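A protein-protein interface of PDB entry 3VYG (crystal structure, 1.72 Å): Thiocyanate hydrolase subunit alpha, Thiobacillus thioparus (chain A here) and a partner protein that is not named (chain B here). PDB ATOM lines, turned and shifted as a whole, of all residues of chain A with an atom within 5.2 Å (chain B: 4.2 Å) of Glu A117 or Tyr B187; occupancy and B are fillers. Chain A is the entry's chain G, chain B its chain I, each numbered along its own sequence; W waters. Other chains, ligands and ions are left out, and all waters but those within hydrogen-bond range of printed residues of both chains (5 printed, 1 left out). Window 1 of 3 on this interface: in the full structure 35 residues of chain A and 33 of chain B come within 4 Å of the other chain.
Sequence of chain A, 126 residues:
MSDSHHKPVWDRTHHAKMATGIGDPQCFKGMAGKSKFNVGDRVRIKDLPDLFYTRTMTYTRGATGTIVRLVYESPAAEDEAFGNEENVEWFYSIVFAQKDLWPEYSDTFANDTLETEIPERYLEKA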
ATOM      1  N   ARG A  55      -2.499  -6.543 -36.327  1.00  0.00           N
ATOM      2  CA  ARG A  55      -3.308  -6.835 -35.100  1.00  0.00           C
ATOM      3  C   ARG A  55      -4.650  -6.109 -35.131  1.00  0.00           C
ATOM      4  O   ARG A  55      -5.322  -5.955 -34.050  1.00  0.00           O
ATOM      5  CB  ARG A  55      -2.524  -6.385 -33.832  1.00  0.00           C
ATOM      6  CG  ARG A  55      -1.242  -7.285 -33.709  1.00  0.00           C
ATOM      7  CD  ARG A  55      -0.608  -7.193 -32.292  1.00  0.00           C
ATOM      8  NE  ARG A  55      -1.352  -7.886 -31.262  1.00  0.00           N
ATOM      9  CZ  ARG A  55      -1.321  -9.217 -31.091  1.00  0.00           C
ATOM     10  NH1 ARG A  55      -0.543 -10.003 -31.914  1.00  0.00           N
ATOM     11  NH2 ARG A  55      -2.007  -9.708 -30.090  1.00  0.00           N
ATOM     12  N   VAL A  71      -5.500   5.557 -25.504  1.00  0.00           N
ATOM     13  CA  VAL A  71      -4.995   4.718 -24.472  1.00  0.00           C
ATOM     14  C   VAL A  71      -3.508   4.957 -24.189  1.00  0.00           C
ATOM     15  O   VAL A  71      -3.128   4.872 -23.010  1.00  0.00           O
ATOM     16  CB  VAL A  71      -5.303   3.205 -24.722  1.00  0.00           C
ATOM     17  CG1 VAL A  71      -6.821   2.993 -24.451  1.00  0.00           C
ATOM     18  CG2 VAL A  71      -4.880   2.751 -26.166  1.00  0.00           C
ATOM     19  N   TYR A  72      -2.699   5.158 -25.226  1.00  0.00           N
ATOM     20  CA  TYR A  72      -1.212   5.281 -25.108  1.00  0.00           C
ATOM     21  C   TYR A  72      -0.691   5.521 -26.472  1.00  0.00           C
ATOM     22  O   TYR A  72      -1.498   5.560 -27.464  1.00  0.00           O
ATOM     23  CB  TYR A  72      -0.509   4.077 -24.420  1.00  0.00           C
ATOM     24  CG  TYR A  72      -0.936   2.779 -25.090  1.00  0.00           C
ATOM     25  CD1 TYR A  72      -0.421   2.423 -26.363  1.00  0.00           C
ATOM     26  CD2 TYR A  72      -1.892   1.995 -24.437  1.00  0.00           C
ATOM     27  CE1 TYR A  72      -0.897   1.206 -26.974  1.00  0.00           C
ATOM     28  CE2 TYR A  72      -2.369   0.799 -25.047  1.00  0.00           C
ATOM     29  CZ  TYR A  72      -1.807   0.459 -26.253  1.00  0.00           C
ATOM     30  OH  TYR A  72      -2.328  -0.652 -26.832  1.00  0.00           O
ATOM     31  N   PHE A  91      -2.860   5.207 -30.135  1.00  0.00           N
ATOM     32  CA  PHE A  91      -3.761   4.065 -30.073  1.00  0.00           C
ATOM     33  C   PHE A  91      -5.057   4.480 -29.420  1.00  0.00           C
ATOM     34  O   PHE A  91      -5.074   5.243 -28.393  1.00  0.00           O
ATOM     35  CB  PHE A  91      -3.134   2.889 -29.269  1.00  0.00           C
ATOM     36  CG  PHE A  91      -2.158   2.078 -30.103  1.00  0.00           C
ATOM     37  CD1 PHE A  91      -0.954   2.616 -30.573  1.00  0.00           C
ATOM     38  CD2 PHE A  91      -2.386   0.695 -30.296  1.00  0.00           C
ATOM     39  CE1 PHE A  91      -0.023   1.834 -31.258  1.00  0.00           C
ATOM     40  CE2 PHE A  91      -1.440  -0.105 -30.930  1.00  0.00           C
ATOM     41  CZ  PHE A  91      -0.296   0.425 -31.424  1.00  0.00           C
ATOM     42  N   TYR A  92      -6.165   3.940 -29.978  1.00  0.00           N
ATOM     43  CA  TYR A  92      -7.496   4.320 -29.527  1.00  0.00           C
ATOM     44  C   TYR A  92      -8.303   3.106 -29.105  1.00  0.00           C
ATOM     45  O   TYR A  92      -8.160   2.040 -29.714  1.00  0.00           O
ATOM     46  CB  TYR A  92      -8.221   4.983 -30.680  1.00  0.00           C
ATOM     47  CG  TYR A  92      -7.563   6.250 -31.195  1.00  0.00           C
ATOM     48  CD1 TYR A  92      -7.953   7.493 -30.647  1.00  0.00           C
ATOM     49  CD2 TYR A  92      -6.570   6.181 -32.157  1.00  0.00           C
ATOM     50  CE1 TYR A  92      -7.360   8.718 -31.141  1.00  0.00           C
ATOM     51  CE2 TYR A  92      -5.912   7.385 -32.689  1.00  0.00           C
ATOM     52  CZ  TYR A  92      -6.364   8.626 -32.140  1.00  0.00           C
ATOM     53  OH  TYR A  92      -5.786   9.711 -32.689  1.00  0.00           O
ATOM     54  N   SER A  93      -9.084   3.217 -28.020  1.00  0.00           N
ATOM     55  CA  SER A  93     -10.003   2.147 -27.653  1.00  0.00           C
ATOM     56  C   SER A  93     -11.310   2.504 -28.256  1.00  0.00           C
ATOM     57  O   SER A  93     -11.834   3.618 -28.071  1.00  0.00           O
ATOM     58  CB  SER A  93     -10.149   2.052 -26.105  1.00  0.00           C
ATOM     59  OG  SER A  93     -10.640   0.702 -25.815  1.00  0.00           O
ATOM     60  N   ILE A  94     -11.889   1.572 -29.035  1.00  0.00           N
ATOM     61  CA  ILE A  94     -13.083   1.861 -29.903  1.00  0.00           C
ATOM     62  C   ILE A  94     -14.158   0.878 -29.494  1.00  0.00           C
ATOM     63  O   ILE A  94     -13.871  -0.320 -29.360  1.00  0.00           O
ATOM     64  CB  ILE A  94     -12.840   1.489 -31.382  1.00  0.00           C
ATOM     65  CG1 ILE A  94     -11.575   2.169 -31.917  1.00  0.00           C
ATOM     66  CG2 ILE A  94     -14.081   1.873 -32.216  1.00  0.00           C
ATOM     67  CD1 ILE A  94     -11.639   3.539 -31.703  1.00  0.00           C
ATOM     68  N   GLU A 115     -15.342  -3.925 -27.439  1.00  0.00           N
ATOM     69  CA  GLU A 115     -14.354  -2.850 -27.382  1.00  0.00           C
ATOM     70  C   GLU A 115     -12.963  -3.442 -27.597  1.00  0.00           C
ATOM     71  O   GLU A 115     -12.590  -4.502 -27.086  1.00  0.00           O
ATOM     72  CB  GLU A 115     -14.407  -2.231 -25.935  1.00  0.00           C
ATOM     73  CG  GLU A 115     -13.306  -1.159 -25.686  1.00  0.00           C
ATOM     74  CD  GLU A 115     -13.438  -0.432 -24.303  1.00  0.00           C
ATOM     75  OE1 GLU A 115     -14.410  -0.643 -23.565  1.00  0.00           O
ATOM     76  OE2 GLU A 115     -12.567   0.471 -24.036  1.00  0.00           O
ATOM     77  N   THR A 116     -12.223  -2.773 -28.483  1.00  0.00           N
ATOM     78  CA  THR A 116     -10.878  -3.221 -28.793  1.00  0.00           C
ATOM     79  C   THR A 116     -10.003  -2.014 -29.209  1.00  0.00           C
ATOM     80  O   THR A 116     -10.521  -0.891 -29.383  1.00  0.00           O
ATOM     81  CB  THR A 116     -10.946  -4.377 -29.879  1.00  0.00           C
ATOM     82  OG1 THR A 116      -9.705  -5.022 -29.928  1.00  0.00           O
ATOM     83  CG2 THR A 116     -11.259  -3.672 -31.160  1.00  0.00           C
ATOM     84  N   GLU A 117      -8.680  -2.255 -29.308  1.00  0.00           N
ATOM     85  CA  GLU A 117      -7.715  -1.123 -29.573  1.00  0.00           C
ATOM     86  C   GLU A 117      -7.236  -1.104 -31.006  1.00  0.00           C
ATOM     87  O   GLU A 117      -6.848  -2.135 -31.561  1.00  0.00           O
ATOM     88  CB  GLU A 117      -6.555  -1.211 -28.554  1.00  0.00           C
ATOM     89  CG  GLU A 117      -7.050  -0.713 -27.187  1.00  0.00           C
ATOM     90  CD  GLU A 117      -5.962  -0.759 -26.104  1.00  0.00           C
ATOM     91  OE1 GLU A 117      -4.866  -1.193 -26.448  1.00  0.00           O
ATOM     92  OE2 GLU A 117      -6.279  -0.361 -24.948  1.00  0.00           O
ATOM     93  N   ILE A 118      -7.126   0.091 -31.583  1.00  0.00           N
ATOM     94  CA  ILE A 118      -6.704   0.224 -32.973  1.00  0.00           C
ATOM     95  C   ILE A 118      -5.756   1.417 -33.061  1.00  0.00           C
ATOM     96  O   ILE A 118      -6.148   2.509 -32.587  1.00  0.00           O
ATOM     97  CB  ILE A 118      -7.978   0.407 -33.834  1.00  0.00           C
ATOM     98  CG1 ILE A 118      -8.808  -0.918 -33.715  1.00  0.00           C
ATOM     99  CG2 ILE A 118      -7.556   0.484 -35.306  1.00  0.00           C
ATOM    100  CD1 ILE A 118     -10.142  -1.036 -34.553  1.00  0.00           C
ATOM    101  N   PRO A 119      -4.621   1.270 -33.734  1.00  0.00           N
ATOM    102  CA  PRO A 119      -3.779   2.470 -33.973  1.00  0.00           C
ATOM    103  C   PRO A 119      -4.354   3.407 -34.975  1.00  0.00           C
ATOM    104  O   PRO A 119      -5.160   3.044 -35.855  1.00  0.00           O
ATOM    105  CB  PRO A 119      -2.451   1.888 -34.414  1.00  0.00           C
ATOM    106  CG  PRO A 119      -2.866   0.529 -35.140  1.00  0.00           C
ATOM    107  CD  PRO A 119      -3.986   0.018 -34.276  1.00  0.00           C
ATOM    108  N   ARG B 114      -6.033  -1.916 -17.705  1.00  0.00           N
ATOM    109  CA  ARG B 114      -7.254  -1.207 -17.537  1.00  0.00           C
ATOM    110  C   ARG B 114      -8.217  -2.042 -16.728  1.00  0.00           C
ATOM    111  O   ARG B 114      -8.353  -3.269 -16.919  1.00  0.00           O
ATOM    112  CB  ARG B 114      -7.882  -0.894 -18.920  1.00  0.00           C
ATOM    113  CG  ARG B 114      -7.224   0.281 -19.575  1.00  0.00           C
ATOM    114  CD  ARG B 114      -8.052   0.817 -20.741  1.00  0.00           C
ATOM    115  NE  ARG B 114      -9.312   1.352 -20.249  1.00  0.00           N
ATOM    116  CZ  ARG B 114     -10.472   1.287 -20.934  1.00  0.00           C
ATOM    117  NH1 ARG B 114     -10.522   0.733 -22.208  1.00  0.00           N
ATOM    118  NH2 ARG B 114     -11.605   1.755 -20.334  1.00  0.00           N
ATOM    119  N   LEU B 116     -12.195  -2.695 -15.941  1.00  0.00           N
ATOM    120  CA  LEU B 116     -13.507  -2.472 -16.554  1.00  0.00           C
ATOM    121  C   LEU B 116     -14.596  -2.587 -15.499  1.00  0.00           C
ATOM    122  O   LEU B 116     -14.800  -3.672 -14.887  1.00  0.00           O
ATOM    123  CB  LEU B 116     -13.672  -3.560 -17.630  1.00  0.00           C
ATOM    124  CG  LEU B 116     -12.618  -3.489 -18.742  1.00  0.00           C
ATOM    125  CD1 LEU B 116     -12.907  -4.677 -19.652  1.00  0.00           C
ATOM    126  CD2 LEU B 116     -12.659  -2.106 -19.571  1.00  0.00           C
ATOM    127  N   VAL B 126     -13.681 -10.729 -21.037  1.00  0.00           N
ATOM    128  CA  VAL B 126     -12.451 -10.447 -21.759  1.00  0.00           C
ATOM    129  C   VAL B 126     -11.928 -11.662 -22.520  1.00  0.00           C
ATOM    130  O   VAL B 126     -12.083 -12.831 -22.083  1.00  0.00           O
ATOM    131  CB  VAL B 126     -11.374 -10.069 -20.704  1.00  0.00           C
ATOM    132  CG1 VAL B 126     -10.101  -9.572 -21.434  1.00  0.00           C
ATOM    133  CG2 VAL B 126     -11.881  -8.889 -19.830  1.00  0.00           C
ATOM    134  N   PRO B 135      -3.831 -10.516 -18.048  1.00  0.00           N
ATOM    135  CA  PRO B 135      -3.034  -9.621 -17.120  1.00  0.00           C
ATOM    136  C   PRO B 135      -2.247 -10.425 -16.067  1.00  0.00           C
ATOM    137  O   PRO B 135      -2.568 -10.287 -14.876  1.00  0.00           O
ATOM    138  CB  PRO B 135      -4.146  -8.818 -16.472  1.00  0.00           C
ATOM    139  CG  PRO B 135      -5.360  -9.824 -16.359  1.00  0.00           C
ATOM    140  CD  PRO B 135      -5.307 -10.455 -17.802  1.00  0.00           C
ATOM    141  N   ALA B 179     -14.424  -7.359 -24.334  1.00  0.00           N
ATOM    142  CA  ALA B 179     -13.168  -6.610 -24.546  1.00  0.00           C
ATOM    143  C   ALA B 179     -12.155  -7.546 -25.144  1.00  0.00           C
ATOM    144  O   ALA B 179     -11.775  -8.585 -24.534  1.00  0.00           O
ATOM    145  CB  ALA B 179     -12.616  -6.009 -23.171  1.00  0.00           C
ATOM    146  N   SER B 181      -8.432  -8.036 -26.168  1.00  0.00           N
ATOM    147  CA  SER B 181      -7.121  -7.509 -25.722  1.00  0.00           C
ATOM    148  C   SER B 181      -6.082  -7.652 -26.836  1.00  0.00           C
ATOM    149  O   SER B 181      -5.168  -8.473 -26.718  1.00  0.00           O
ATOM    150  CB  SER B 181      -6.612  -8.373 -24.491  1.00  0.00           C
ATOM    151  OG  SER B 181      -7.677  -8.402 -23.603  1.00  0.00           O
ATOM    152  N   ASN B 182      -6.241  -6.885 -27.924  1.00  0.00           N
ATOM    153  CA  ASN B 182      -5.432  -7.141 -29.156  1.00  0.00           C
ATOM    154  C   ASN B 182      -4.199  -6.197 -29.293  1.00  0.00           C
ATOM    155  O   ASN B 182      -3.432  -6.359 -30.231  1.00  0.00           O
ATOM    156  CB  ASN B 182      -6.283  -6.902 -30.424  1.00  0.00           C
ATOM    157  CG  ASN B 182      -6.754  -5.458 -30.559  1.00  0.00           C
ATOM    158  OD1 ASN B 182      -7.068  -4.819 -29.551  1.00  0.00           O
ATOM    159  ND2 ASN B 182      -6.850  -4.953 -31.762  1.00  0.00           N
ATOM    160  N   GLN B 183      -3.913  -5.352 -28.317  1.00  0.00           N
ATOM    161  CA  GLN B 183      -2.681  -4.518 -28.390  1.00  0.00           C
ATOM    162  C   GLN B 183      -2.001  -4.604 -27.061  1.00  0.00           C
ATOM    163  O   GLN B 183      -1.862  -5.712 -26.513  1.00  0.00           O
ATOM    164  CB  GLN B 183      -3.042  -3.042 -28.755  1.00  0.00           C
ATOM    165  CG  GLN B 183      -3.884  -3.016 -30.080  1.00  0.00           C
ATOM    166  CD  GLN B 183      -3.134  -3.303 -31.395  1.00  0.00           C
ATOM    167  OE1 GLN B 183      -1.923  -3.426 -31.459  1.00  0.00           O
ATOM    168  NE2 GLN B 183      -3.935  -3.325 -32.525  1.00  0.00           N
ATOM    169  N   LYS B 184      -1.585  -3.419 -26.538  1.00  0.00           N
ATOM    170  CA  LYS B 184      -0.805  -3.533 -25.284  1.00  0.00           C
ATOM    171  C   LYS B 184      -1.614  -3.447 -24.009  1.00  0.00           C
ATOM    172  O   LYS B 184      -1.025  -3.649 -22.944  1.00  0.00           O
ATOM    173  CB  LYS B 184       0.369  -2.538 -25.247  1.00  0.00           C
ATOM    174  CG  LYS B 184       1.417  -2.882 -26.319  1.00  0.00           C
ATOM    175  CD  LYS B 184       2.582  -1.815 -26.333  1.00  0.00           C
ATOM    176  CE  LYS B 184       3.659  -2.261 -27.325  1.00  0.00           C
ATOM    177  NZ  LYS B 184       4.748  -1.199 -27.452  1.00  0.00           N
ATOM    178  N   THR B 185      -2.917  -3.171 -24.062  1.00  0.00           N
ATOM    179  CA  THR B 185      -3.687  -3.158 -22.803  1.00  0.00           C
ATOM    180  C   THR B 185      -4.088  -4.538 -22.337  1.00  0.00           C
ATOM    181  O   THR B 185      -4.368  -5.421 -23.187  1.00  0.00           O
ATOM    182  CB  THR B 185      -4.911  -2.350 -23.020  1.00  0.00           C
ATOM    183  OG1 THR B 185      -4.532  -0.992 -23.148  1.00  0.00           O
ATOM    184  CG2 THR B 185      -5.978  -2.488 -21.833  1.00  0.00           C
ATOM    185  N   ARG B 186      -4.112  -4.771 -21.027  1.00  0.00           N
ATOM    186  CA  ARG B 186      -4.563  -6.023 -20.421  1.00  0.00           C
ATOM    187  C   ARG B 186      -5.705  -5.530 -19.522  1.00  0.00           C
ATOM    188  O   ARG B 186      -5.634  -4.436 -18.987  1.00  0.00           O
ATOM    189  CB  ARG B 186      -3.460  -6.711 -19.528  1.00  0.00           C
ATOM    190  CG  ARG B 186      -2.245  -7.092 -20.421  1.00  0.00           C
ATOM    191  CD  ARG B 186      -2.671  -8.264 -21.432  1.00  0.00           C
ATOM    192  NE  ARG B 186      -1.510  -8.525 -22.321  1.00  0.00           N
ATOM    193  CZ  ARG B 186      -1.294  -7.930 -23.519  1.00  0.00           C
ATOM    194  NH1 ARG B 186      -2.097  -7.002 -24.091  1.00  0.00           N
ATOM    195  NH2 ARG B 186      -0.173  -8.254 -24.157  1.00  0.00           N
ATOM    196  N   TYR B 187      -6.727  -6.388 -19.367  1.00  0.00           N
ATOM    197  CA  TYR B 187      -7.915  -5.960 -18.594  1.00  0.00           C
ATOM    198  C   TYR B 187      -8.178  -6.864 -17.433  1.00  0.00           C
ATOM    199  O   TYR B 187      -7.940  -8.065 -17.528  1.00  0.00           O
ATOM    200  CB  TYR B 187      -9.234  -6.101 -19.476  1.00  0.00           C
ATOM    201  CG  TYR B 187      -9.227  -5.202 -20.728  1.00  0.00           C
ATOM    202  CD1 TYR B 187      -9.479  -3.840 -20.703  1.00  0.00           C
ATOM    203  CD2 TYR B 187      -8.903  -5.762 -21.939  1.00  0.00           C
ATOM    204  CE1 TYR B 187      -9.555  -3.027 -21.918  1.00  0.00           C
ATOM    205  CE2 TYR B 187      -8.905  -5.012 -23.122  1.00  0.00           C
ATOM    206  CZ  TYR B 187      -9.179  -3.666 -23.119  1.00  0.00           C
ATOM    207  OH  TYR B 187      -9.210  -2.959 -24.261  1.00  0.00           O
ATOM    208  N   ILE B 188      -8.736  -6.279 -16.343  1.00  0.00           N
ATOM    209  CA  ILE B 188      -9.508  -7.098 -15.373  1.00  0.00           C
ATOM    210  C   ILE B 188     -10.900  -6.484 -15.254  1.00  0.00           C
ATOM    211  O   ILE B 188     -11.094  -5.306 -15.545  1.00  0.00           O
ATOM    212  CB  ILE B 188      -8.867  -7.205 -13.973  1.00  0.00           C
ATOM    213  CG1 ILE B 188      -8.550  -5.777 -13.448  1.00  0.00           C
ATOM    214  CG2 ILE B 188      -7.601  -8.058 -14.059  1.00  0.00           C
ATOM    215  CD1 ILE B 188      -8.076  -5.885 -11.866  1.00  0.00           C
HETATM  216  O   HOH W   1     -14.220   0.966 -21.427  1.00  0.00           O
HETATM  217  O   HOH W   2      -2.907  -3.317 -35.631  1.00  0.00           O
HETATM  218  O   HOH W   3      -5.008  -4.524 -25.786  1.00  0.00           O
HETATM  219  O   HOH W   4      -8.766  -0.411 -24.159  1.00  0.00           O
HETATM  220  O   HOH W   5      -7.752  -3.902 -26.410  1.00  0.00           O
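The backbone carbonyl oxygen (O) of Glu A117 lies within hydrogen-bond range of the side-chain amide nitrogen (NE2) of Gln B183, at 3.3 Å. OD1 of Asn B182 is in hydrogen-bond range of OG1 of Thr A116. The side-chain amide nitrogen (ND2) of Asn B182 is in hydrogen-bond range of the backbone carbonyl oxygen (O) of Glu A117, at 2.8 Å. NE of Arg A55 sits at hydrogen-bond distance from O of Asn B182, 2.8 Å away. The guanidinium group (NH1) of Arg B114 lies within salt-bridge range of the side-chain carboxylate (OE2) of Glu A115 (2.8 Å). OH of Tyr A72 sits at hydrogen-bond distance from N of Lys B184. OG1 of Thr B185 lies within hydrogen-bond range of OE2 of Glu A117. The backbone carbonyl oxygen (O) of Arg A55 is in hydrogen-bond range of the side-chain amide nitrogen (NE2) of Gln B183 (3.3 Å).
The backbone carbonyl oxygen (O) of Gln B183 lies within hydrogen-bond range of the guanidinium group (NH1) of Arg B186 (2.8 Å). The backbone carbonyl oxygen (O) of Tyr A72 is in hydrogen-bond range of the backbone NH (N) of Phe A91 (3.0 Å). N of Arg B114 lies within hydrogen-bond range of O of Arg B186. The side-chain amide nitrogen of Asn B182 sits close to the side-chain amide nitrogen of Gln B183 (3.4 Å). The side-chain carboxylate (OE1) of Glu A117 sits at hydrogen-bond distance from the side-chain hydroxyl (OH) of Tyr A72 (2.6 Å). O of Arg B114 is in hydrogen-bond range of N of Ile B188 (3.1 Å).
Among the printed residues, pairs that only touch across the chains: Tyr A72 with Gln B183 (3.1 Å), Tyr A72 with Thr B185 (3.4 Å), Phe A91 with Gln B183 (3.4 Å), Ser A93 with Arg B114 (3.6 Å), Glu A115 with Ala B179 (3.4 Å), Glu A117 with Lys B184 (3.97 Å), Glu A117 with Tyr B187 (3.98 Å) and Pro A119 with Gln B183 (3.8 Å).
Of the printed residues of chain B, Glu A117 touches Asn B182, Gln B183, Lys B184, Thr B185 and Tyr B187. Printed residues of chain A within 4 Å of Tyr B187: Glu A117 (3.98 Å). Of the printed residues of chain A, Gln B183 touches Arg A55, Tyr A72, Phe A91, Glu A117 and Pro A119. Printed residues of chain A within 4 Å of Ala B179: Glu A115. The nearest residue of chain A that does not touch Tyr B187 is Ser A93 (4.2 Å).
Of the 12 printed residues of chain A, 8 touch a printed residue of chain B. Printed residues of chain A that touch a printed residue of chain B: Arg A55, Tyr A72, Phe A91, Ser A93, Glu A115, Thr A116, Glu A117 and Pro A119. Hydrophobic or aromatic side chains of chain A that line the printed part of chain B: Tyr A72, Phe A91 and Pro A119. Of the 13 printed residues of chain B, 7 touch a printed residue of chain A. Hydrophobic or aromatic side chains of chain B that line the printed part of chain A: Tyr B187. Among the printed residues, 16 pairs touch across the chains. Among the printed residues, Asp or Glu carboxylates within 4 Å of a Lys or Arg side-chain nitrogen of the other chain: Glu A115 with Arg B114 (2.8 Å).
Water W4 lies within hydrogen-bond range of OH of Tyr B187 (2.6 Å), OE2 of Glu A117 (2.6 Å), OG of Ser A93 (2.7 Å) and NH1 of Arg B114 (2.9 Å). Water W1 lies within hydrogen-bond range of the side-chain carboxylate (OE1) of Glu A115 (2.7 Å) and the guanidinium group (NH2) of Arg B114 (2.9 Å). Water W5 lies within hydrogen-bond range of OH of Tyr B187 (2.8 Å), OD1 of Asn B182 (3.3 Å) and N of Glu A117 (3.5 Å). Water W3 lies within hydrogen-bond range of O of Thr B185 (2.8 Å), N of Gln B183 (2.9 Å), OE1 of Glu A117 (3.4 Å) and N of Asn B182 (3.4 Å). Water W2 lies within hydrogen-bond range of NE2 of Gln B183 (3.3 Å) and N of Arg A55 (3.3 Å).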
